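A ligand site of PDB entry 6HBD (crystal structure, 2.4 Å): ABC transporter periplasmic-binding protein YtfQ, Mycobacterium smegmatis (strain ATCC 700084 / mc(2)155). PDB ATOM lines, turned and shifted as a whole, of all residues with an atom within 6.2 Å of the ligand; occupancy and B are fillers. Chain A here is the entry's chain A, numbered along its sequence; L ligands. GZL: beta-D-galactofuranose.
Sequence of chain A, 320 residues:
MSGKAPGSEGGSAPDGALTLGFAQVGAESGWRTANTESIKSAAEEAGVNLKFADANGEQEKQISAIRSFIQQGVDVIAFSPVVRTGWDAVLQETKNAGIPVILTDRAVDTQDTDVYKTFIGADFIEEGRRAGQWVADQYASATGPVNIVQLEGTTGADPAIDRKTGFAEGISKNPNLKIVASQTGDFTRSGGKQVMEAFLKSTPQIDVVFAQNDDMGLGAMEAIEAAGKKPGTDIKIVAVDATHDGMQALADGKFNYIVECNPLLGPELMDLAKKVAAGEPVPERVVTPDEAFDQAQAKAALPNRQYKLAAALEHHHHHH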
ATOM      1  N   GLU A  28     -16.150   7.556 -14.965  1.00  0.00           N
ATOM      2  CA  GLU A  28     -15.285   8.611 -15.511  1.00  0.00           C
ATOM      3  C   GLU A  28     -15.757  10.094 -15.276  1.00  0.00           C
ATOM      4  O   GLU A  28     -14.916  10.985 -15.349  1.00  0.00           O
ATOM      5  CB  GLU A  28     -15.019   8.367 -17.032  1.00  0.00           C
ATOM      6  CG  GLU A  28     -16.136   8.686 -18.020  1.00  0.00           C
ATOM      7  CD  GLU A  28     -17.380   7.822 -17.925  1.00  0.00           C
ATOM      8  OE1 GLU A  28     -18.431   8.263 -18.440  1.00  0.00           O
ATOM      9  OE2 GLU A  28     -17.307   6.724 -17.335  1.00  0.00           O
ATOM     10  N   SER A  29     -17.080  10.364 -15.080  1.00  0.00           N
ATOM     11  CA  SER A  29     -17.602  11.712 -14.845  1.00  0.00           C
ATOM     12  C   SER A  29     -18.734  11.737 -13.843  1.00  0.00           C
ATOM     13  O   SER A  29     -19.286  10.688 -13.492  1.00  0.00           O
ATOM     14  CB  SER A  29     -18.127  12.284 -16.153  1.00  0.00           C
ATOM     15  OG  SER A  29     -19.220  11.507 -16.634  1.00  0.00           O
ATOM     16  N   GLY A  30     -19.123  12.962 -13.455  1.00  0.00           N
ATOM     17  CA  GLY A  30     -20.262  13.230 -12.583  1.00  0.00           C
ATOM     18  C   GLY A  30     -21.543  12.728 -13.211  1.00  0.00           C
ATOM     19  O   GLY A  30     -22.367  12.060 -12.553  1.00  0.00           O
ATOM     20  N   TRP A  31     -21.696  13.019 -14.514  1.00  0.00           N
ATOM     21  CA  TRP A  31     -22.843  12.543 -15.303  1.00  0.00           C
ATOM     22  C   TRP A  31     -22.990  11.018 -15.142  1.00  0.00           C
ATOM     23  O   TRP A  31     -24.110  10.518 -15.034  1.00  0.00           O
ATOM     24  CB  TRP A  31     -22.646  12.875 -16.805  1.00  0.00           C
ATOM     25  CG  TRP A  31     -23.891  12.718 -17.639  1.00  0.00           C
ATOM     26  CD1 TRP A  31     -24.720  13.703 -18.082  1.00  0.00           C
ATOM     27  CD2 TRP A  31     -24.453  11.482 -18.089  1.00  0.00           C
ATOM     28  NE1 TRP A  31     -25.770  13.160 -18.784  1.00  0.00           N
ATOM     29  CE2 TRP A  31     -25.653  11.792 -18.760  1.00  0.00           C
ATOM     30  CE3 TRP A  31     -24.050  10.152 -18.026  1.00  0.00           C
ATOM     31  CZ2 TRP A  31     -26.425  10.833 -19.379  1.00  0.00           C
ATOM     32  CZ3 TRP A  31     -24.852   9.193 -18.585  1.00  0.00           C
ATOM     33  CH2 TRP A  31     -26.037   9.534 -19.241  1.00  0.00           C
ATOM     34  N   ARG A  32     -21.880  10.281 -15.197  1.00  0.00           N
ATOM     35  CA  ARG A  32     -21.870   8.818 -15.091  1.00  0.00           C
ATOM     36  C   ARG A  32     -22.304   8.357 -13.699  1.00  0.00           C
ATOM     37  O   ARG A  32     -23.126   7.437 -13.558  1.00  0.00           O
ATOM     38  CB  ARG A  32     -20.463   8.280 -15.367  1.00  0.00           C
ATOM     39  CG  ARG A  32     -20.442   6.889 -15.947  1.00  0.00           C
ATOM     40  CD  ARG A  32     -20.672   6.930 -17.428  1.00  0.00           C
ATOM     41  NE  ARG A  32     -21.833   6.177 -17.850  1.00  0.00           N
ATOM     42  CZ  ARG A  32     -22.369   6.243 -19.051  1.00  0.00           C
ATOM     43  NH1 ARG A  32     -23.445   5.516 -19.343  1.00  0.00           N
ATOM     44  NH2 ARG A  32     -21.865   7.062 -19.979  1.00  0.00           N
ATOM     45  N   SER A  80     -24.391   0.785 -21.846  1.00  0.00           N
ATOM     46  CA  SER A  80     -24.014   2.037 -22.474  1.00  0.00           C
ATOM     47  C   SER A  80     -22.780   1.744 -23.333  1.00  0.00           C
ATOM     48  O   SER A  80     -21.682   1.677 -22.788  1.00  0.00           O
ATOM     49  CB  SER A  80     -23.716   3.093 -21.414  1.00  0.00           C
ATOM     50  OG  SER A  80     -22.959   4.154 -21.965  1.00  0.00           O
ATOM     51  N   THR A 104     -28.493   2.650 -23.716  1.00  0.00           N
ATOM     52  CA  THR A 104     -28.726   3.859 -22.928  1.00  0.00           C
ATOM     53  C   THR A 104     -27.514   4.824 -23.052  1.00  0.00           C
ATOM     54  O   THR A 104     -26.363   4.399 -22.934  1.00  0.00           O
ATOM     55  CB  THR A 104     -29.130   3.549 -21.455  1.00  0.00           C
ATOM     56  OG1 THR A 104     -28.014   3.577 -20.573  1.00  0.00           O
ATOM     57  CG2 THR A 104     -29.893   2.264 -21.296  1.00  0.00           C
ATOM     58  N   ASP A 105     -27.817   6.099 -23.380  1.00  0.00           N
ATOM     59  CA  ASP A 105     -26.921   7.249 -23.508  1.00  0.00           C
ATOM     60  C   ASP A 105     -25.773   7.142 -24.540  1.00  0.00           C
ATOM     61  O   ASP A 105     -25.073   8.126 -24.750  1.00  0.00           O
ATOM     62  CB  ASP A 105     -26.376   7.651 -22.135  1.00  0.00           C
ATOM     63  CG  ASP A 105     -25.430   6.710 -21.437  1.00  0.00           C
ATOM     64  OD1 ASP A 105     -24.212   6.728 -21.763  1.00  0.00           O
ATOM     65  OD2 ASP A 105     -25.884   5.968 -20.527  1.00  0.00           O
ATOM     66  N   ARG A 106     -25.613   5.996 -25.223  1.00  0.00           N
ATOM     67  CA  ARG A 106     -24.624   5.785 -26.267  1.00  0.00           C
ATOM     68  C   ARG A 106     -25.189   4.776 -27.275  1.00  0.00           C
ATOM     69  O   ARG A 106     -25.867   3.835 -26.886  1.00  0.00           O
ATOM     70  CB  ARG A 106     -23.311   5.259 -25.679  1.00  0.00           C
ATOM     71  CG  ARG A 106     -22.294   6.367 -25.472  1.00  0.00           C
ATOM     72  CD  ARG A 106     -21.203   6.032 -24.477  1.00  0.00           C
ATOM     73  NE  ARG A 106     -20.620   7.219 -23.880  1.00  0.00           N
ATOM     74  CZ  ARG A 106     -19.566   7.230 -23.075  1.00  0.00           C
ATOM     75  NH1 ARG A 106     -18.956   6.091 -22.754  1.00  0.00           N
ATOM     76  NH2 ARG A 106     -19.088   8.366 -22.601  1.00  0.00           N
ATOM     77  N   GLY A 121     -31.428   8.281 -25.163  1.00  0.00           N
ATOM     78  CA  GLY A 121     -30.274   9.177 -25.057  1.00  0.00           C
ATOM     79  C   GLY A 121     -30.628  10.554 -25.546  1.00  0.00           C
ATOM     80  O   GLY A 121     -31.785  10.773 -25.863  1.00  0.00           O
ATOM     81  N   ALA A 122     -29.646  11.475 -25.668  1.00  0.00           N
ATOM     82  CA  ALA A 122     -29.932  12.832 -26.136  1.00  0.00           C
ATOM     83  C   ALA A 122     -29.493  12.999 -27.596  1.00  0.00           C
ATOM     84  O   ALA A 122     -28.928  12.070 -28.158  1.00  0.00           O
ATOM     85  CB  ALA A 122     -29.242  13.832 -25.244  1.00  0.00           C
ATOM     86  N   PHE A 124     -26.921  14.456 -29.310  1.00  0.00           N
ATOM     87  CA  PHE A 124     -25.524  14.918 -29.136  1.00  0.00           C
ATOM     88  C   PHE A 124     -25.109  15.951 -30.163  1.00  0.00           C
ATOM     89  O   PHE A 124     -24.438  16.920 -29.801  1.00  0.00           O
ATOM     90  CB  PHE A 124     -24.585  13.721 -29.218  1.00  0.00           C
ATOM     91  CG  PHE A 124     -24.944  12.653 -28.213  1.00  0.00           C
ATOM     92  CD1 PHE A 124     -25.194  12.973 -26.893  1.00  0.00           C
ATOM     93  CD2 PHE A 124     -25.141  11.338 -28.614  1.00  0.00           C
ATOM     94  CE1 PHE A 124     -25.552  12.009 -25.986  1.00  0.00           C
ATOM     95  CE2 PHE A 124     -25.472  10.365 -27.696  1.00  0.00           C
ATOM     96  CZ  PHE A 124     -25.688  10.706 -26.382  1.00  0.00           C
ATOM     97  N   GLU A 127     -26.637  19.054 -29.030  1.00  0.00           N
ATOM     98  CA  GLU A 127     -25.943  19.537 -27.831  1.00  0.00           C
ATOM     99  C   GLU A 127     -24.710  20.327 -28.320  1.00  0.00           C
ATOM    100  O   GLU A 127     -24.539  21.487 -27.920  1.00  0.00           O
ATOM    101  CB  GLU A 127     -25.537  18.394 -26.905  1.00  0.00           C
ATOM    102  CG  GLU A 127     -26.706  17.749 -26.202  1.00  0.00           C
ATOM    103  CD  GLU A 127     -26.378  16.493 -25.427  1.00  0.00           C
ATOM    104  OE1 GLU A 127     -25.262  15.969 -25.585  1.00  0.00           O
ATOM    105  OE2 GLU A 127     -27.243  16.044 -24.632  1.00  0.00           O
ATOM    106  N   PRO A 159     -21.394  10.100 -28.177  1.00  0.00           N
ATOM    107  CA  PRO A 159     -21.509  11.556 -27.886  1.00  0.00           C
ATOM    108  C   PRO A 159     -20.315  12.424 -28.337  1.00  0.00           C
ATOM    109  O   PRO A 159     -20.516  13.581 -28.745  1.00  0.00           O
ATOM    110  CB  PRO A 159     -21.704  11.598 -26.367  1.00  0.00           C
ATOM    111  CG  PRO A 159     -21.301  10.271 -25.859  1.00  0.00           C
ATOM    112  CD  PRO A 159     -21.528   9.295 -26.935  1.00  0.00           C
ATOM    113  N   ARG A 163     -20.956  15.310 -30.880  1.00  0.00           N
ATOM    114  CA  ARG A 163     -20.771  16.673 -30.332  1.00  0.00           C
ATOM    115  C   ARG A 163     -19.742  17.441 -31.128  1.00  0.00           C
ATOM    116  O   ARG A 163     -19.911  18.654 -31.315  1.00  0.00           O
ATOM    117  CB  ARG A 163     -20.376  16.649 -28.850  1.00  0.00           C
ATOM    118  CG  ARG A 163     -21.563  16.371 -27.950  1.00  0.00           C
ATOM    119  CD  ARG A 163     -21.169  15.890 -26.577  1.00  0.00           C
ATOM    120  NE  ARG A 163     -22.332  15.442 -25.818  1.00  0.00           N
ATOM    121  CZ  ARG A 163     -22.296  14.894 -24.614  1.00  0.00           C
ATOM    122  NH1 ARG A 163     -21.133  14.719 -23.999  1.00  0.00           N
ATOM    123  NH2 ARG A 163     -23.419  14.530 -24.004  1.00  0.00           N
ATOM    124  N   ASP A 186     -10.627  11.900 -22.564  1.00  0.00           N
ATOM    125  CA  ASP A 186     -11.256  10.683 -22.036  1.00  0.00           C
ATOM    126  C   ASP A 186     -12.536  10.888 -21.150  1.00  0.00           C
ATOM    127  O   ASP A 186     -12.945   9.937 -20.455  1.00  0.00           O
ATOM    128  CB  ASP A 186     -10.197   9.871 -21.255  1.00  0.00           C
ATOM    129  CG  ASP A 186     -10.378   8.361 -21.357  1.00  0.00           C
ATOM    130  OD1 ASP A 186     -10.627   7.856 -22.485  1.00  0.00           O
ATOM    131  OD2 ASP A 186     -10.265   7.675 -20.308  1.00  0.00           O
ATOM    132  N   PHE A 187     -13.190  12.096 -21.243  1.00  0.00           N
ATOM    133  CA  PHE A 187     -14.358  12.471 -20.460  1.00  0.00           C
ATOM    134  C   PHE A 187     -14.060  12.498 -18.906  1.00  0.00           C
ATOM    135  O   PHE A 187     -14.992  12.300 -18.093  1.00  0.00           O
ATOM    136  CB  PHE A 187     -15.604  11.592 -20.821  1.00  0.00           C
ATOM    137  CG  PHE A 187     -16.384  11.892 -22.086  1.00  0.00           C
ATOM    138  CD1 PHE A 187     -16.627  13.197 -22.478  1.00  0.00           C
ATOM    139  CD2 PHE A 187     -17.080  10.889 -22.736  1.00  0.00           C
ATOM    140  CE1 PHE A 187     -17.487  13.489 -23.536  1.00  0.00           C
ATOM    141  CE2 PHE A 187     -17.902  11.183 -23.833  1.00  0.00           C
ATOM    142  CZ  PHE A 187     -18.094  12.484 -24.233  1.00  0.00           C
ATOM    143  N   GLN A 212     -16.443  18.852 -24.218  1.00  0.00           N
ATOM    144  CA  GLN A 212     -17.567  17.988 -24.601  1.00  0.00           C
ATOM    145  C   GLN A 212     -18.226  17.352 -23.385  1.00  0.00           C
ATOM    146  O   GLN A 212     -19.207  16.610 -23.533  1.00  0.00           O
ATOM    147  CB  GLN A 212     -17.123  16.927 -25.621  1.00  0.00           C
ATOM    148  CG  GLN A 212     -16.918  17.520 -27.009  1.00  0.00           C
ATOM    149  CD  GLN A 212     -16.350  16.513 -27.965  1.00  0.00           C
ATOM    150  OE1 GLN A 212     -16.329  15.300 -27.715  1.00  0.00           O
ATOM    151  NE2 GLN A 212     -15.844  16.991 -29.088  1.00  0.00           N
ATOM    152  N   ASN A 213     -17.689  17.626 -22.190  1.00  0.00           N
ATOM    153  CA  ASN A 213     -18.240  17.098 -20.945  1.00  0.00           C
ATOM    154  C   ASN A 213     -17.728  18.072 -19.904  1.00  0.00           C
ATOM    155  O   ASN A 213     -16.553  18.399 -19.941  1.00  0.00           O
ATOM    156  CB  ASN A 213     -17.763  15.664 -20.800  1.00  0.00           C
ATOM    157  CG  ASN A 213     -17.270  15.246 -19.474  1.00  0.00           C
ATOM    158  OD1 ASN A 213     -16.071  15.209 -19.222  1.00  0.00           O
ATOM    159  ND2 ASN A 213     -18.200  14.890 -18.600  1.00  0.00           N
ATOM    160  N   ASP A 214     -18.616  18.631 -19.053  1.00  0.00           N
ATOM    161  CA  ASP A 214     -18.159  19.665 -18.139  1.00  0.00           C
ATOM    162  C   ASP A 214     -17.105  19.189 -17.113  1.00  0.00           C
ATOM    163  O   ASP A 214     -16.402  20.046 -16.593  1.00  0.00           O
ATOM    164  CB  ASP A 214     -19.293  20.466 -17.451  1.00  0.00           C
ATOM    165  CG  ASP A 214     -20.505  19.789 -16.906  1.00  0.00           C
ATOM    166  OD1 ASP A 214     -20.413  18.606 -16.538  1.00  0.00           O
ATOM    167  OD2 ASP A 214     -21.565  20.469 -16.806  1.00  0.00           O
ATOM    168  N   ASP A 215     -16.903  17.853 -16.900  1.00  0.00           N
ATOM    169  CA  ASP A 215     -15.796  17.401 -16.050  1.00  0.00           C
ATOM    170  C   ASP A 215     -14.466  17.822 -16.712  1.00  0.00           C
ATOM    171  O   ASP A 215     -13.629  18.418 -16.046  1.00  0.00           O
ATOM    172  CB  ASP A 215     -15.809  15.890 -15.820  1.00  0.00           C
ATOM    173  CG  ASP A 215     -16.861  15.465 -14.851  1.00  0.00           C
ATOM    174  OD1 ASP A 215     -18.037  15.902 -15.009  1.00  0.00           O
ATOM    175  OD2 ASP A 215     -16.532  14.697 -13.932  1.00  0.00           O
ATOM    176  N   VAL A 240     -20.965  20.583 -22.190  1.00  0.00           N
ATOM    177  CA  VAL A 240     -22.178  19.768 -22.289  1.00  0.00           C
ATOM    178  C   VAL A 240     -22.260  18.909 -21.020  1.00  0.00           C
ATOM    179  O   VAL A 240     -21.215  18.500 -20.511  1.00  0.00           O
ATOM    180  CB  VAL A 240     -22.143  18.934 -23.595  1.00  0.00           C
ATOM    181  CG1 VAL A 240     -23.339  17.989 -23.689  1.00  0.00           C
ATOM    182  CG2 VAL A 240     -22.085  19.844 -24.818  1.00  0.00           C
ATOM    183  N   ASP A 241     -23.475  18.666 -20.521  1.00  0.00           N
ATOM    184  CA  ASP A 241     -23.851  17.907 -19.315  1.00  0.00           C
ATOM    185  C   ASP A 241     -24.587  18.751 -18.308  1.00  0.00           C
ATOM    186  O   ASP A 241     -25.716  18.312 -18.041  1.00  0.00           O
ATOM    187  CB  ASP A 241     -22.722  17.166 -18.592  1.00  0.00           C
ATOM    188  CG  ASP A 241     -22.203  15.915 -19.249  1.00  0.00           C
ATOM    189  OD1 ASP A 241     -22.745  15.521 -20.318  1.00  0.00           O
ATOM    190  OD2 ASP A 241     -21.256  15.302 -18.681  1.00  0.00           O
ATOM    191  N   CYS A 261     -27.378  17.583 -20.475  1.00  0.00           N
ATOM    192  CA  CYS A 261     -27.557  16.217 -20.962  1.00  0.00           C
ATOM    193  C   CYS A 261     -28.061  15.507 -19.717  1.00  0.00           C
ATOM    194  O   CYS A 261     -27.347  15.461 -18.715  1.00  0.00           O
ATOM    195  CB  CYS A 261     -26.261  15.600 -21.476  1.00  0.00           C
ATOM    196  SG  CYS A 261     -26.459  13.904 -22.047  1.00  0.00           S
HETATM  197  C6  GZL L   1     -23.964  11.106 -22.937  1.00  0.00           C
HETATM  198  C5  GZL L   1     -23.121  10.173 -22.102  1.00  0.00           C
HETATM  199  C4  GZL L   1     -21.742  10.742 -21.824  1.00  0.00           C
HETATM  200  C3  GZL L   1     -21.725  12.067 -21.058  1.00  0.00           C
HETATM  201  C2  GZL L   1     -20.338  12.025 -20.434  1.00  0.00           C
HETATM  202  O6  GZL L   1     -25.174  10.449 -23.318  1.00  0.00           O
HETATM  203  O5  GZL L   1     -23.033   8.871 -22.698  1.00  0.00           O
HETATM  204  O4  GZL L   1     -21.007   9.847 -20.960  1.00  0.00           O
HETATM  205  O3  GZL L   1     -21.875  13.222 -21.858  1.00  0.00           O
HETATM  206  C1  GZL L   1     -20.275  10.571 -19.970  1.00  0.00           C
HETATM  207  O2  GZL L   1     -20.175  12.903 -19.334  1.00  0.00           O
HETATM  208  O1  GZL L   1     -18.916  10.310 -20.032  1.00  0.00           O
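O2 of the ligand sits at hydrogen-bond distance from OD2 of Asp 241 (2.7 Å). The backbone carbonyl oxygen (O) of Asp 105 is in hydrogen-bond range of an oxygen (O6) of the ligand (2.7 Å). The side-chain carboxylate of Asp 105 lies within hydrogen-bond range of an oxygen (O5) of the ligand, 2.6 Å away. An oxygen (O4) of the ligand is in hydrogen-bond range of the guanidinium group of Arg 32 (3.1 Å). The side-chain hydroxyl (OG) of Ser 29 sits at hydrogen-bond distance from an oxygen (O2) of the ligand. NH1 of Arg 163 is in hydrogen-bond range of O3 of the ligand, at 2.7 Å. The guanidinium group (NH2) of Arg 106 sits at hydrogen-bond distance from an oxygen (O4) of the ligand (2.9 Å). The side-chain carboxylate (OE1) of Glu 28 is in hydrogen-bond range of an oxygen (O1) of the ligand (2.6 Å). The side-chain amide nitrogen (ND2) of Asn 213 is in hydrogen-bond range of an oxygen (O2) of the ligand.
The guanidinium group of Arg 32 is in salt-bridge range of the side-chain carboxylate of Glu 28 (3.95 Å). SG of Cys 261 sits close to OE2 of Glu 127 (3.4 Å). The backbone carbonyl oxygen (O) of Gln 212 is in hydrogen-bond range of the guanidinium group (NH1) of Arg 163. The side-chain hydroxyl (OG1) of Thr 104 is in hydrogen-bond range of the side-chain carboxylate (OD2) of Asp 105 (3.2 Å). The backbone NH (N) of Arg 32 sits at hydrogen-bond distance from the side-chain hydroxyl (OG) of Ser 29, at 3.3 Å. The side-chain carboxylate of Asp 241 lies within salt-bridge range of the guanidinium group of Arg 163 (3.9 Å). The backbone carbonyl oxygen (O) of Asp 241 lies within hydrogen-bond range of the backbone NH (N) of Cys 261 (3.0 Å). NH1 of Arg 32 lies within salt-bridge range of OD2 of Asp 105 (2.7 Å).
Residues that only touch the ligand: Phe 124 (3.1 Å), Phe 187 (3.3 Å), Trp 31 (3.5 Å), Cys 261 (3.9 Å) and Pro 159 (3.9 Å). Of the 24 residues printed, 13 come within 4 Å of the ligand.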
